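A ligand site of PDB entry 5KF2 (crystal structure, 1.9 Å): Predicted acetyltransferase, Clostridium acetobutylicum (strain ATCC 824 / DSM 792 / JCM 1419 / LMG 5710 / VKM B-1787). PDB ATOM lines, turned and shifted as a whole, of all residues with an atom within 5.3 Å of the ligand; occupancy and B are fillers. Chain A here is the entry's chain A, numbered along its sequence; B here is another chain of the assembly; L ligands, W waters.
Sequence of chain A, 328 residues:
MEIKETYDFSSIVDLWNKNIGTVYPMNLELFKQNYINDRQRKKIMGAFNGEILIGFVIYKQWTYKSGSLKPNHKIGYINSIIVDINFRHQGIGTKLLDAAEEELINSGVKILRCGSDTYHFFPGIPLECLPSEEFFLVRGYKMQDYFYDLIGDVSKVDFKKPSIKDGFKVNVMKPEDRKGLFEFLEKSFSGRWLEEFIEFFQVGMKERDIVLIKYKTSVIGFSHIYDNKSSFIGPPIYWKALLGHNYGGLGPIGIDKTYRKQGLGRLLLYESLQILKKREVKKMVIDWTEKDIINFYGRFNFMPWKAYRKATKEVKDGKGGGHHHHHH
ND1 of His 89 sits at hydrogen-bond distance from O3 of the ligand (2.8 Å).
The side-chain sulfur (SG) of Cys 129 lies close to an oxygen (O16) of the ligand (3.3 Å).
A nitrogen (N7) of the ligand lies within hydrogen-bond range of the backbone carbonyl oxygen (O) of Ile 81, 2.8 Å away.
The backbone NH (N) of Thr 94 lies within hydrogen-bond range of an oxygen (O9) of the ligand (2.9 Å).
A nitrogen (N1) of the ligand lies close to the side-chain amide oxygen of Asn 295 of chain B (2.9 Å).
The backbone NH of Gly 91 lies within hydrogen-bond range of an oxygen (O8) of the ligand (3.0 Å).
The backbone NH (N) of Gln 90 lies within hydrogen-bond range of an oxygen (O8) of the ligand.
The backbone NH (N) of His 89 sits at hydrogen-bond distance from an oxygen (O12) of the ligand, 3.0 Å away.
N of Ile 81 is in hydrogen-bond range of O17 of the ligand, 3.2 Å away.
The backbone NH of Gly 93 lies within hydrogen-bond range of an oxygen (O11) of the ligand (2.9 Å).
The side-chain hydroxyl (OG1) of Thr 94 sits at hydrogen-bond distance from an oxygen (O9) of the ligand, at 2.5 Å.
O15 of the ligand is in hydrogen-bond range of N of Val 83 (2.9 Å).
O of Val 83 is in hydrogen-bond range of NE of Arg 88 (2.8 Å).
O of Ile 78 sits at hydrogen-bond distance from N of Gly 115 (2.8 Å).
OD1 of Asn 79 is in hydrogen-bond range of OG of Ser 80 (2.8 Å).
The side-chain hydroxyl (OG) of Ser 132 is in hydrogen-bond range of the backbone carbonyl oxygen (O) of Cys 129.
O of Ile 78 touches C23 of the ligand, 3.5 Å away.
Ser 80 touches the ligand.
CA of Ile 82 touches O15 of the ligand (3.4 Å).
Arg 88 touches the ligand.
Ile 92 touches the ligand (N to O11, 3.7 Å).
Cys 114 touches the ligand (CB to C23, 3.96 Å).
N of Gly 115 touches C23 of the ligand (3.8 Å).
Pro 126 touches the ligand (CD to S1, 3.8 Å).
Pro 131 touches the ligand.
CB of Ser 132 touches O16 of the ligand (3.5 Å).
Glu 134 touches the ligand.
Phe 135 touches the ligand.
Val 138 touches the ligand (CG2 to O1, 3.8 Å).
Hydrophobic or aromatic side chains within 4 Å of the ligand: Ile 81, Ile 82, Val 83, His 89, Pro 126, Pro 131, Phe 135 and Val 138.
22 residues have an atom within 4 Å of the ligand: Ile 78, Ser 80, Ile 81, Ile 82, Val 83, Arg 88, His 89, Gln 90, Gly 91, Ile 92, Gly 93, Thr 94, Cys 114, Gly 115, Pro 126, Cys 129, Pro 131, Ser 132, Glu 134, Phe 135, Val 138 and Asn 295 of chain B.
Along chain A the residues within 4 Å of the ligand span positions 78 to 138.
Water W9 lies within hydrogen-bond range of O3 of the ligand (2.5 Å), O of His 89 (3.4 Å) and N of Gly 91 (3.5 Å).
Water W4 lies within hydrogen-bond range of an oxygen (O3) of the ligand (2.9 Å) and the backbone carbonyl oxygen of His 89 (3.1 Å).
Water W6 bridges a nitrogen (N1) of the ligand (3.0 Å) and the backbone carbonyl oxygen (O) of Pro 131 (3.0 Å).
Water W3 lies within hydrogen-bond range of NE2 of His 89 (2.8 Å) and N3 of the ligand (3.5 Å).
Water W11 lies within hydrogen-bond range of NH2 of Arg 88 and O14 of the ligand.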
ATOM      1  N   ILE A  20       3.711  -5.906   9.546  1.00  0.00           N
ATOM      2  CA  ILE A  20       4.654  -5.102  10.290  1.00  0.00           C
ATOM      3  C   ILE A  20       5.963  -5.778  10.713  1.00  0.00           C
ATOM      4  O   ILE A  20       6.747  -5.211  11.469  1.00  0.00           O
ATOM      5  CB  ILE A  20       3.956  -4.375  11.460  1.00  0.00           C
ATOM      6  CG1 ILE A  20       3.579  -5.339  12.594  1.00  0.00           C
ATOM      7  CG2 ILE A  20       2.740  -3.583  10.949  1.00  0.00           C
ATOM      8  CD1 ILE A  20       3.091  -4.598  13.834  1.00  0.00           C
ATOM      9  N   ILE A  78      -6.035  -1.377  24.355  1.00  0.00           N
ATOM     10  CA  ILE A  78      -5.861  -1.947  23.027  1.00  0.00           C
ATOM     11  C   ILE A  78      -4.397  -2.390  22.911  1.00  0.00           C
ATOM     12  O   ILE A  78      -3.510  -1.546  22.779  1.00  0.00           O
ATOM     13  CB  ILE A  78      -6.178  -0.895  21.949  1.00  0.00           C
ATOM     14  CG1 ILE A  78      -7.525  -0.208  22.255  1.00  0.00           C
ATOM     15  CG2 ILE A  78      -6.079  -1.516  20.569  1.00  0.00           C
ATOM     16  CD1 ILE A  78      -8.699  -1.162  22.293  1.00  0.00           C
ATOM     17  N   ASN A  79      -4.172  -3.691  23.019  1.00  0.00           N
ATOM     18  CA  ASN A  79      -2.857  -4.270  23.070  1.00  0.00           C
ATOM     19  C   ASN A  79      -2.256  -4.120  21.667  1.00  0.00           C
ATOM     20  O   ASN A  79      -1.120  -3.735  21.549  1.00  0.00           O
ATOM     21  CB  ASN A  79      -2.986  -5.745  23.471  1.00  0.00           C
ATOM     22  CG  ASN A  79      -1.782  -6.609  23.087  1.00  0.00           C
ATOM     23  OD1 ASN A  79      -1.698  -7.128  21.966  1.00  0.00           O
ATOM     24  ND2 ASN A  79      -0.897  -6.846  24.041  1.00  0.00           N
ATOM     25  N   SER A  80      -3.064  -4.419  20.658  1.00  0.00           N
ATOM     26  CA  SER A  80      -2.681  -4.289  19.264  1.00  0.00           C
ATOM     27  C   SER A  80      -3.891  -4.393  18.351  1.00  0.00           C
ATOM     28  O   SER A  80      -4.919  -4.945  18.740  1.00  0.00           O
ATOM     29  CB  SER A  80      -1.707  -5.396  18.894  1.00  0.00           C
ATOM     30  OG  SER A  80      -2.195  -6.688  19.201  1.00  0.00           O
ATOM     31  N   ILE A  81      -3.741  -3.839  17.158  1.00  0.00           N
ATOM     32  CA  ILE A  81      -4.737  -3.928  16.091  1.00  0.00           C
ATOM     33  C   ILE A  81      -4.047  -3.802  14.737  1.00  0.00           C
ATOM     34  O   ILE A  81      -3.242  -2.884  14.521  1.00  0.00           O
ATOM     35  CB  ILE A  81      -5.863  -2.850  16.239  1.00  0.00           C
ATOM     36  CG1 ILE A  81      -6.914  -3.055  15.136  1.00  0.00           C
ATOM     37  CG2 ILE A  81      -5.325  -1.448  16.243  1.00  0.00           C
ATOM     38  CD1 ILE A  81      -8.140  -2.161  15.311  1.00  0.00           C
ATOM     39  N   ILE A  82      -4.298  -4.768  13.860  1.00  0.00           N
ATOM     40  CA  ILE A  82      -3.734  -4.803  12.525  1.00  0.00           C
ATOM     41  C   ILE A  82      -4.835  -5.281  11.555  1.00  0.00           C
ATOM     42  O   ILE A  82      -5.479  -6.305  11.789  1.00  0.00           O
ATOM     43  CB  ILE A  82      -2.488  -5.667  12.405  1.00  0.00           C
ATOM     44  CG1 ILE A  82      -1.448  -5.414  13.525  1.00  0.00           C
ATOM     45  CG2 ILE A  82      -1.883  -5.530  11.013  1.00  0.00           C
ATOM     46  CD1 ILE A  82      -0.317  -6.420  13.575  1.00  0.00           C
ATOM     47  N   VAL A  83      -5.064  -4.488  10.512  1.00  0.00           N
ATOM     48  CA  VAL A  83      -5.811  -4.914   9.335  1.00  0.00           C
ATOM     49  C   VAL A  83      -4.840  -5.248   8.206  1.00  0.00           C
ATOM     50  O   VAL A  83      -3.836  -4.542   7.966  1.00  0.00           O
ATOM     51  CB  VAL A  83      -6.815  -3.819   8.965  1.00  0.00           C
ATOM     52  CG1 VAL A  83      -7.475  -4.134   7.629  1.00  0.00           C
ATOM     53  CG2 VAL A  83      -7.846  -3.727  10.073  1.00  0.00           C
ATOM     54  N   PHE A  87      -6.621  -5.089   2.601  1.00  0.00           N
ATOM     55  CA  PHE A  87      -7.991  -4.824   2.999  1.00  0.00           C
ATOM     56  C   PHE A  87      -8.165  -3.518   3.766  1.00  0.00           C
ATOM     57  O   PHE A  87      -9.129  -3.367   4.501  1.00  0.00           O
ATOM     58  CB  PHE A  87      -8.538  -6.013   3.819  1.00  0.00           C
ATOM     59  CG  PHE A  87      -8.531  -7.305   3.046  1.00  0.00           C
ATOM     60  CD1 PHE A  87      -9.680  -7.717   2.352  1.00  0.00           C
ATOM     61  CD2 PHE A  87      -7.400  -8.066   2.963  1.00  0.00           C
ATOM     62  CE1 PHE A  87      -9.693  -8.890   1.620  1.00  0.00           C
ATOM     63  CE2 PHE A  87      -7.406  -9.230   2.212  1.00  0.00           C
ATOM     64  CZ  PHE A  87      -8.557  -9.656   1.558  1.00  0.00           C
ATOM     65  N   ARG A  88      -7.267  -2.551   3.566  1.00  0.00           N
ATOM     66  CA  ARG A  88      -7.302  -1.262   4.260  1.00  0.00           C
ATOM     67  C   ARG A  88      -8.366  -0.337   3.714  1.00  0.00           C
ATOM     68  O   ARG A  88      -8.835  -0.541   2.602  1.00  0.00           O
ATOM     69  CB  ARG A  88      -5.968  -0.522   4.090  1.00  0.00           C
ATOM     70  CG  ARG A  88      -4.811  -1.259   4.737  1.00  0.00           C
ATOM     71  CD  ARG A  88      -4.707  -1.121   6.239  1.00  0.00           C
ATOM     72  NE  ARG A  88      -3.669  -2.032   6.729  1.00  0.00           N
ATOM     73  CZ  ARG A  88      -2.363  -1.800   6.725  1.00  0.00           C
ATOM     74  NH1 ARG A  88      -1.524  -2.728   7.136  1.00  0.00           N
ATOM     75  NH2 ARG A  88      -1.888  -0.614   6.350  1.00  0.00           N
ATOM     76  N   HIS A  89      -8.748   0.630   4.538  1.00  0.00           N
ATOM     77  CA  HIS A  89      -9.706   1.632   4.130  1.00  0.00           C
ATOM     78  C   HIS A  89     -11.034   1.119   3.660  1.00  0.00           C
ATOM     79  O   HIS A  89     -11.671   1.758   2.823  1.00  0.00           O
ATOM     80  CB  HIS A  89      -9.084   2.605   3.105  1.00  0.00           C
ATOM     81  CG  HIS A  89      -7.974   3.423   3.691  1.00  0.00           C
ATOM     82  ND1 HIS A  89      -8.218   4.548   4.451  1.00  0.00           N
ATOM     83  CD2 HIS A  89      -6.633   3.253   3.662  1.00  0.00           C
ATOM     84  CE1 HIS A  89      -7.061   5.070   4.809  1.00  0.00           C
ATOM     85  NE2 HIS A  89      -6.089   4.298   4.360  1.00  0.00           N
ATOM     86  N   GLN A  90     -11.489   0.034   4.281  1.00  0.00           N
ATOM     87  CA  GLN A  90     -12.782  -0.543   4.000  1.00  0.00           C
ATOM     88  C   GLN A  90     -13.640  -0.533   5.264  1.00  0.00           C
ATOM     89  O   GLN A  90     -14.700  -1.164   5.241  1.00  0.00           O
ATOM     90  CB  GLN A  90     -12.608  -1.990   3.529  1.00  0.00           C
ATOM     91  CG  GLN A  90     -11.845  -2.148   2.224  1.00  0.00           C
ATOM     92  CD  GLN A  90     -11.905  -3.567   1.696  1.00  0.00           C
ATOM     93  OE1 GLN A  90     -12.742  -4.350   2.106  1.00  0.00           O
ATOM     94  NE2 GLN A  90     -10.983  -3.921   0.849  1.00  0.00           N
ATOM     95  N   GLY A  91     -13.229   0.165   6.335  1.00  0.00           N
ATOM     96  CA  GLY A  91     -13.933   0.141   7.603  1.00  0.00           C
ATOM     97  C   GLY A  91     -13.686  -1.010   8.568  1.00  0.00           C
ATOM     98  O   GLY A  91     -14.338  -1.057   9.628  1.00  0.00           O
ATOM     99  N   ILE A  92     -12.777  -1.940   8.239  1.00  0.00           N
ATOM    100  CA  ILE A  92     -12.553  -3.116   9.051  1.00  0.00           C
ATOM    101  C   ILE A  92     -11.912  -2.813  10.389  1.00  0.00           C
ATOM    102  O   ILE A  92     -12.360  -3.348  11.397  1.00  0.00           O
ATOM    103  CB  ILE A  92     -11.733  -4.188   8.330  1.00  0.00           C
ATOM    104  CG1 ILE A  92     -12.519  -4.701   7.128  1.00  0.00           C
ATOM    105  CG2 ILE A  92     -11.378  -5.375   9.221  1.00  0.00           C
ATOM    106  CD1 ILE A  92     -11.641  -5.534   6.209  1.00  0.00           C
ATOM    107  N   GLY A  93     -10.871  -1.976  10.369  1.00  0.00           N
ATOM    108  CA  GLY A  93     -10.278  -1.426  11.595  1.00  0.00           C
ATOM    109  C   GLY A  93     -11.306  -0.761  12.514  1.00  0.00           C
ATOM    110  O   GLY A  93     -11.342  -1.016  13.720  1.00  0.00           O
ATOM    111  N   THR A  94     -12.129   0.137  11.958  1.00  0.00           N
ATOM    112  CA  THR A  94     -13.277   0.669  12.703  1.00  0.00           C
ATOM    113  C   THR A  94     -14.239  -0.321  13.394  1.00  0.00           C
ATOM    114  O   THR A  94     -14.582  -0.170  14.573  1.00  0.00           O
ATOM    115  CB  THR A  94     -14.083   1.661  11.806  1.00  0.00           C
ATOM    116  OG1 THR A  94     -13.174   2.684  11.371  1.00  0.00           O
ATOM    117  CG2 THR A  94     -15.198   2.360  12.611  1.00  0.00           C
ATOM    118  N   LYS A  95     -14.625  -1.363  12.669  1.00  0.00           N
ATOM    119  CA  LYS A  95     -15.523  -2.376  13.206  1.00  0.00           C
ATOM    120  C   LYS A  95     -14.889  -3.228  14.298  1.00  0.00           C
ATOM    121  O   LYS A  95     -15.525  -3.512  15.308  1.00  0.00           O
ATOM    122  CB  LYS A  95     -15.974  -3.295  12.086  1.00  0.00           C
ATOM    123  CG  LYS A  95     -16.857  -2.548  11.106  1.00  0.00           C
ATOM    124  CD  LYS A  95     -17.382  -3.450  10.025  1.00  0.00           C
ATOM    125  CE  LYS A  95     -18.425  -2.657   9.254  1.00  0.00           C
ATOM    126  NZ  LYS A  95     -18.446  -3.257   7.896  1.00  0.00           N
ATOM    127  N   CYS A 114      -3.797   3.051  24.333  1.00  0.00           N
ATOM    128  CA  CYS A 114      -3.121   2.344  23.289  1.00  0.00           C
ATOM    129  C   CYS A 114      -1.820   1.757  23.794  1.00  0.00           C
ATOM    130  O   CYS A 114      -0.885   2.493  24.131  1.00  0.00           O
ATOM    131  CB  CYS A 114      -2.828   3.282  22.119  1.00  0.00           C
ATOM    132  SG  CYS A 114      -4.276   3.851  21.177  1.00  0.00           S
ATOM    133  N   GLY A 115      -1.730   0.429  23.742  1.00  0.00           N
ATOM    134  CA  GLY A 115      -0.661  -0.306  24.415  1.00  0.00           C
ATOM    135  C   GLY A 115      -0.540   0.045  25.872  1.00  0.00           C
ATOM    136  O   GLY A 115      -1.523   0.446  26.536  1.00  0.00           O
ATOM    137  N   PHE A 122       3.609  -3.068  22.943  1.00  0.00           N
ATOM    138  CA  PHE A 122       4.017  -1.710  22.699  1.00  0.00           C
ATOM    139  C   PHE A 122       3.763  -0.785  23.928  1.00  0.00           C
ATOM    140  O   PHE A 122       2.677  -0.776  24.479  1.00  0.00           O
ATOM    141  CB  PHE A 122       3.225  -1.140  21.536  1.00  0.00           C
ATOM    142  CG  PHE A 122       3.163  -1.989  20.291  1.00  0.00           C
ATOM    143  CD1 PHE A 122       4.305  -2.342  19.608  1.00  0.00           C
ATOM    144  CD2 PHE A 122       1.950  -2.428  19.793  1.00  0.00           C
ATOM    145  CE1 PHE A 122       4.252  -3.109  18.460  1.00  0.00           C
ATOM    146  CE2 PHE A 122       1.868  -3.154  18.613  1.00  0.00           C
ATOM    147  CZ  PHE A 122       3.016  -3.497  17.949  1.00  0.00           C
ATOM    148  N   GLY A 124       3.163   2.254  23.570  1.00  0.00           N
ATOM    149  CA  GLY A 124       2.272   3.247  22.968  1.00  0.00           C
ATOM    150  C   GLY A 124       2.169   3.029  21.461  1.00  0.00           C
ATOM    151  O   GLY A 124       2.630   1.999  20.980  1.00  0.00           O
ATOM    152  N   ILE A 125       1.600   3.979  20.707  1.00  0.00           N
ATOM    153  CA  ILE A 125       1.576   3.830  19.236  1.00  0.00           C
ATOM    154  C   ILE A 125       2.982   3.958  18.639  1.00  0.00           C
ATOM    155  O   ILE A 125       3.592   4.986  18.750  1.00  0.00           O
ATOM    156  CB  ILE A 125       0.720   4.913  18.563  1.00  0.00           C
ATOM    157  CG1 ILE A 125      -0.693   4.874  19.205  1.00  0.00           C
ATOM    158  CG2 ILE A 125       0.751   4.735  17.055  1.00  0.00           C
ATOM    159  CD1 ILE A 125      -1.608   6.017  18.766  1.00  0.00           C
ATOM    160  N   PRO A 126       3.519   2.871  18.061  1.00  0.00           N
ATOM    161  CA  PRO A 126       4.889   2.995  17.529  1.00  0.00           C
ATOM    162  C   PRO A 126       4.996   4.084  16.452  1.00  0.00           C
ATOM    163  O   PRO A 126       4.071   4.252  15.644  1.00  0.00           O
ATOM    164  CB  PRO A 126       5.162   1.615  16.907  1.00  0.00           C
ATOM    165  CG  PRO A 126       4.228   0.715  17.668  1.00  0.00           C
ATOM    166  CD  PRO A 126       2.987   1.529  17.801  1.00  0.00           C
ATOM    167  N   CYS A 129       4.210   2.995  13.099  1.00  0.00           N
ATOM    168  CA  CYS A 129       2.751   3.077  12.888  1.00  0.00           C
ATOM    169  C   CYS A 129       2.168   4.480  13.025  1.00  0.00           C
ATOM    170  O   CYS A 129       0.995   4.635  13.367  1.00  0.00           O
ATOM    171  CB  CYS A 129       2.067   2.164  13.915  1.00  0.00           C
ATOM    172  SG  CYS A 129       2.628   0.461  13.784  1.00  0.00           S
ATOM    173  N   PRO A 131       1.079   6.631  10.955  1.00  0.00           N
ATOM    174  CA  PRO A 131      -0.184   6.948  10.275  1.00  0.00           C
ATOM    175  C   PRO A 131      -1.439   6.533  11.036  1.00  0.00           C
ATOM    176  O   PRO A 131      -2.510   7.131  10.833  1.00  0.00           O
ATOM    177  CB  PRO A 131      -0.090   6.165   8.950  1.00  0.00           C
ATOM    178  CG  PRO A 131       1.388   6.126   8.676  1.00  0.00           C
ATOM    179  CD  PRO A 131       1.984   5.864  10.061  1.00  0.00           C
ATOM    180  N   SER A 132      -1.323   5.513  11.873  1.00  0.00           N
ATOM    181  CA  SER A 132      -2.430   5.077  12.702  1.00  0.00           C
ATOM    182  C   SER A 132      -2.837   6.103  13.748  1.00  0.00           C
ATOM    183  O   SER A 132      -3.951   6.018  14.242  1.00  0.00           O
ATOM    184  CB  SER A 132      -2.129   3.717  13.365  1.00  0.00           C
ATOM    185  OG  SER A 132      -1.304   3.896  14.521  1.00  0.00           O
ATOM    186  N   GLU A 134      -3.713   9.020  13.277  1.00  0.00           N
ATOM    187  CA  GLU A 134      -4.881   9.678  12.707  1.00  0.00           C
ATOM    188  C   GLU A 134      -6.105   8.790  12.825  1.00  0.00           C
ATOM    189  O   GLU A 134      -7.199   9.276  13.092  1.00  0.00           O
ATOM    190  CB  GLU A 134      -4.595  10.040  11.238  1.00  0.00           C
ATOM    191  CG  GLU A 134      -5.484  11.096  10.629  1.00  0.00           C
ATOM    192  CD  GLU A 134      -5.347  12.412  11.358  1.00  0.00           C
ATOM    193  OE1 GLU A 134      -4.218  12.809  11.724  1.00  0.00           O
ATOM    194  OE2 GLU A 134      -6.412  13.024  11.581  1.00  0.00           O
ATOM    195  N   PHE A 135      -5.947   7.481  12.611  1.00  0.00           N
ATOM    196  CA  PHE A 135      -7.014   6.527  12.918  1.00  0.00           C
ATOM    197  C   PHE A 135      -7.556   6.656  14.339  1.00  0.00           C
ATOM    198  O   PHE A 135      -8.771   6.693  14.525  1.00  0.00           O
ATOM    199  CB  PHE A 135      -6.548   5.101  12.607  1.00  0.00           C
ATOM    200  CG  PHE A 135      -7.484   4.002  13.006  1.00  0.00           C
ATOM    201  CD1 PHE A 135      -8.560   3.644  12.193  1.00  0.00           C
ATOM    202  CD2 PHE A 135      -7.240   3.247  14.146  1.00  0.00           C
ATOM    203  CE1 PHE A 135      -9.397   2.590  12.554  1.00  0.00           C
ATOM    204  CE2 PHE A 135      -8.063   2.203  14.497  1.00  0.00           C
ATOM    205  CZ  PHE A 135      -9.144   1.855  13.686  1.00  0.00           C
ATOM    206  N   PHE A 136      -6.664   6.695  15.338  1.00  0.00           N
ATOM    207  CA  PHE A 136      -7.077   6.777  16.721  1.00  0.00           C
ATOM    208  C   PHE A 136      -7.666   8.147  16.990  1.00  0.00           C
ATOM    209  O   PHE A 136      -8.677   8.251  17.676  1.00  0.00           O
ATOM    210  CB  PHE A 136      -5.916   6.424  17.675  1.00  0.00           C
ATOM    211  CG  PHE A 136      -5.541   4.962  17.616  1.00  0.00           C
ATOM    212  CD1 PHE A 136      -6.404   3.990  18.124  1.00  0.00           C
ATOM    213  CD2 PHE A 136      -4.352   4.539  17.017  1.00  0.00           C
ATOM    214  CE1 PHE A 136      -6.042   2.653  18.101  1.00  0.00           C
ATOM    215  CE2 PHE A 136      -4.013   3.203  16.948  1.00  0.00           C
ATOM    216  CZ  PHE A 136      -4.849   2.266  17.507  1.00  0.00           C
ATOM    217  N   VAL A 138      -9.312  10.144  14.974  1.00  0.00           N
ATOM    218  CA  VAL A 138     -10.664  10.156  14.422  1.00  0.00           C
ATOM    219  C   VAL A 138     -11.658   9.490  15.389  1.00  0.00           C
ATOM    220  O   VAL A 138     -12.818   9.882  15.417  1.00  0.00           O
ATOM    221  CB  VAL A 138     -10.674   9.422  13.056  1.00  0.00           C
ATOM    222  CG1 VAL A 138     -12.056   8.915  12.696  1.00  0.00           C
ATOM    223  CG2 VAL A 138     -10.169  10.343  11.945  1.00  0.00           C
ATOM    224  N   ASN B 295       1.410   8.106   3.464  1.00  0.00           N
ATOM    225  CA  ASN B 295       0.330   7.183   3.076  1.00  0.00           C
ATOM    226  C   ASN B 295       0.396   6.753   1.602  1.00  0.00           C
ATOM    227  O   ASN B 295       0.004   5.628   1.284  1.00  0.00           O
ATOM    228  CB  ASN B 295      -1.046   7.790   3.360  1.00  0.00           C
ATOM    229  CG  ASN B 295      -1.422   7.769   4.837  1.00  0.00           C
ATOM    230  OD1 ASN B 295      -2.297   8.523   5.293  1.00  0.00           O
ATOM    231  ND2 ASN B 295      -0.787   6.882   5.587  1.00  0.00           N
HETATM  232  N1  LIG L   1      -3.908   7.841   7.552  1.00  0.00           N
HETATM  233  C1  LIG L   1      -4.845   8.741   7.927  1.00  0.00           C
HETATM  234  N2  LIG L   1      -6.065   8.376   8.400  1.00  0.00           N
HETATM  235  C2  LIG L   1      -6.373   7.053   8.520  1.00  0.00           C
HETATM  236  C3  LIG L   1      -5.403   6.000   8.123  1.00  0.00           C
HETATM  237  C4  LIG L   1      -4.120   6.492   7.593  1.00  0.00           C
HETATM  238  N3  LIG L   1      -3.246   5.512   7.246  1.00  0.00           N
HETATM  239  N4  LIG L   1      -5.961   4.781   8.301  1.00  0.00           N
HETATM  240  C5  LIG L   1      -7.218   5.028   8.805  1.00  0.00           C
HETATM  241  N5  LIG L   1      -7.441   6.375   8.938  1.00  0.00           N
HETATM  242  C6  LIG L   1      -8.678   7.081   9.385  1.00  0.00           C
HETATM  243  C7  LIG L   1      -9.426   7.571   8.137  1.00  0.00           C
HETATM  244  O1  LIG L   1     -10.251   8.701   8.473  1.00  0.00           O
HETATM  245  C8  LIG L   1     -10.279   6.389   7.770  1.00  0.00           C
HETATM  246  O2  LIG L   1     -11.360   6.749   6.907  1.00  0.00           O
HETATM  247  P1  LIG L   1     -11.162   6.724   5.290  1.00  0.00           P
HETATM  248  O3  LIG L   1     -10.840   5.310   4.907  1.00  0.00           O
HETATM  249  O4  LIG L   1     -12.584   7.164   4.958  1.00  0.00           O
HETATM  250  O5  LIG L   1     -10.025   7.696   5.091  1.00  0.00           O
HETATM  251  C9  LIG L   1     -10.675   5.937   9.179  1.00  0.00           C
HETATM  252  O6  LIG L   1      -9.504   6.086   9.955  1.00  0.00           O
HETATM  253  C10 LIG L   1     -11.178   4.522   9.360  1.00  0.00           C
HETATM  254  O7  LIG L   1     -10.299   3.629   8.705  1.00  0.00           O
HETATM  255  P2  LIG L   1     -10.615   2.090   8.592  1.00  0.00           P
HETATM  256  O8  LIG L   1     -10.842   1.733   7.148  1.00  0.00           O
HETATM  257  O9  LIG L   1     -11.613   1.703   9.610  1.00  0.00           O
HETATM  258  O10 LIG L   1      -9.116   1.529   8.991  1.00  0.00           O
HETATM  259  P3  LIG L   1      -8.412   0.207   8.439  1.00  0.00           P
HETATM  260  O11 LIG L   1      -9.186  -1.064   8.234  1.00  0.00           O
HETATM  261  O12 LIG L   1      -7.568   0.740   7.319  1.00  0.00           O
HETATM  262  O13 LIG L   1      -7.406  -0.055   9.655  1.00  0.00           O
HETATM  263  C11 LIG L   1      -5.326   0.371  10.854  1.00  0.00           C
HETATM  264  C12 LIG L   1      -6.618   0.977  10.303  1.00  0.00           C
HETATM  265  C13 LIG L   1      -5.703  -0.799  11.773  1.00  0.00           C
HETATM  266  C14 LIG L   1      -4.593   1.445  11.649  1.00  0.00           C
HETATM  267  C15 LIG L   1      -4.455  -0.148   9.714  1.00  0.00           C
HETATM  268  O14 LIG L   1      -3.998   0.934   8.882  1.00  0.00           O
HETATM  269  C16 LIG L   1      -3.278  -0.981  10.134  1.00  0.00           C
HETATM  270  O15 LIG L   1      -3.403  -2.171  10.432  1.00  0.00           O
HETATM  271  N6  LIG L   1      -2.094  -0.341  10.130  1.00  0.00           N
HETATM  272  C17 LIG L   1      -0.898  -1.086  10.454  1.00  0.00           C
HETATM  273  C18 LIG L   1      -0.843  -1.510  11.908  1.00  0.00           C
HETATM  274  C19 LIG L   1      -1.006  -0.365  12.904  1.00  0.00           C
HETATM  275  O16 LIG L   1      -0.425   0.713  12.686  1.00  0.00           O
HETATM  276  N7  LIG L   1      -1.683  -0.592  14.036  1.00  0.00           N
HETATM  277  C20 LIG L   1      -1.751   0.357  15.105  1.00  0.00           C
HETATM  278  C21 LIG L   1      -0.575   0.119  16.062  1.00  0.00           C
HETATM  279  S1  LIG L   1      -0.773   0.811  17.679  1.00  0.00           S
HETATM  280  C22 LIG L   1      -1.676  -0.289  18.560  1.00  0.00           C
HETATM  281  O17 LIG L   1      -1.995  -1.363  18.098  1.00  0.00           O
HETATM  282  C23 LIG L   1      -2.097   0.050  19.950  1.00  0.00           C
HETATM  283  O   HOH W   1     -14.636   5.938   3.849  1.00  0.00           O
HETATM  284  O   HOH W   2       0.251   2.521  10.620  1.00  0.00           O
HETATM  285  O   HOH W   3      -3.737   5.652   3.814  1.00  0.00           O
HETATM  286  O   HOH W   4     -11.978   4.782   2.245  1.00  0.00           O
HETATM  287  O   HOH W   5      -8.517  10.442   8.579  1.00  0.00           O
HETATM  288  O   HOH W   6      -1.931   9.525   9.078  1.00  0.00           O
HETATM  289  O   HOH W   7     -13.237   8.643   7.233  1.00  0.00           O
HETATM  290  O   HOH W   8      -5.445   2.216   7.184  1.00  0.00           O
HETATM  291  O   HOH W   9     -12.318   3.458   5.738  1.00  0.00           O
HETATM  292  O   HOH W  10      -1.620   2.688   8.860  1.00  0.00           O
HETATM  293  O   HOH W  11      -3.260   1.850   5.586  1.00  0.00           O
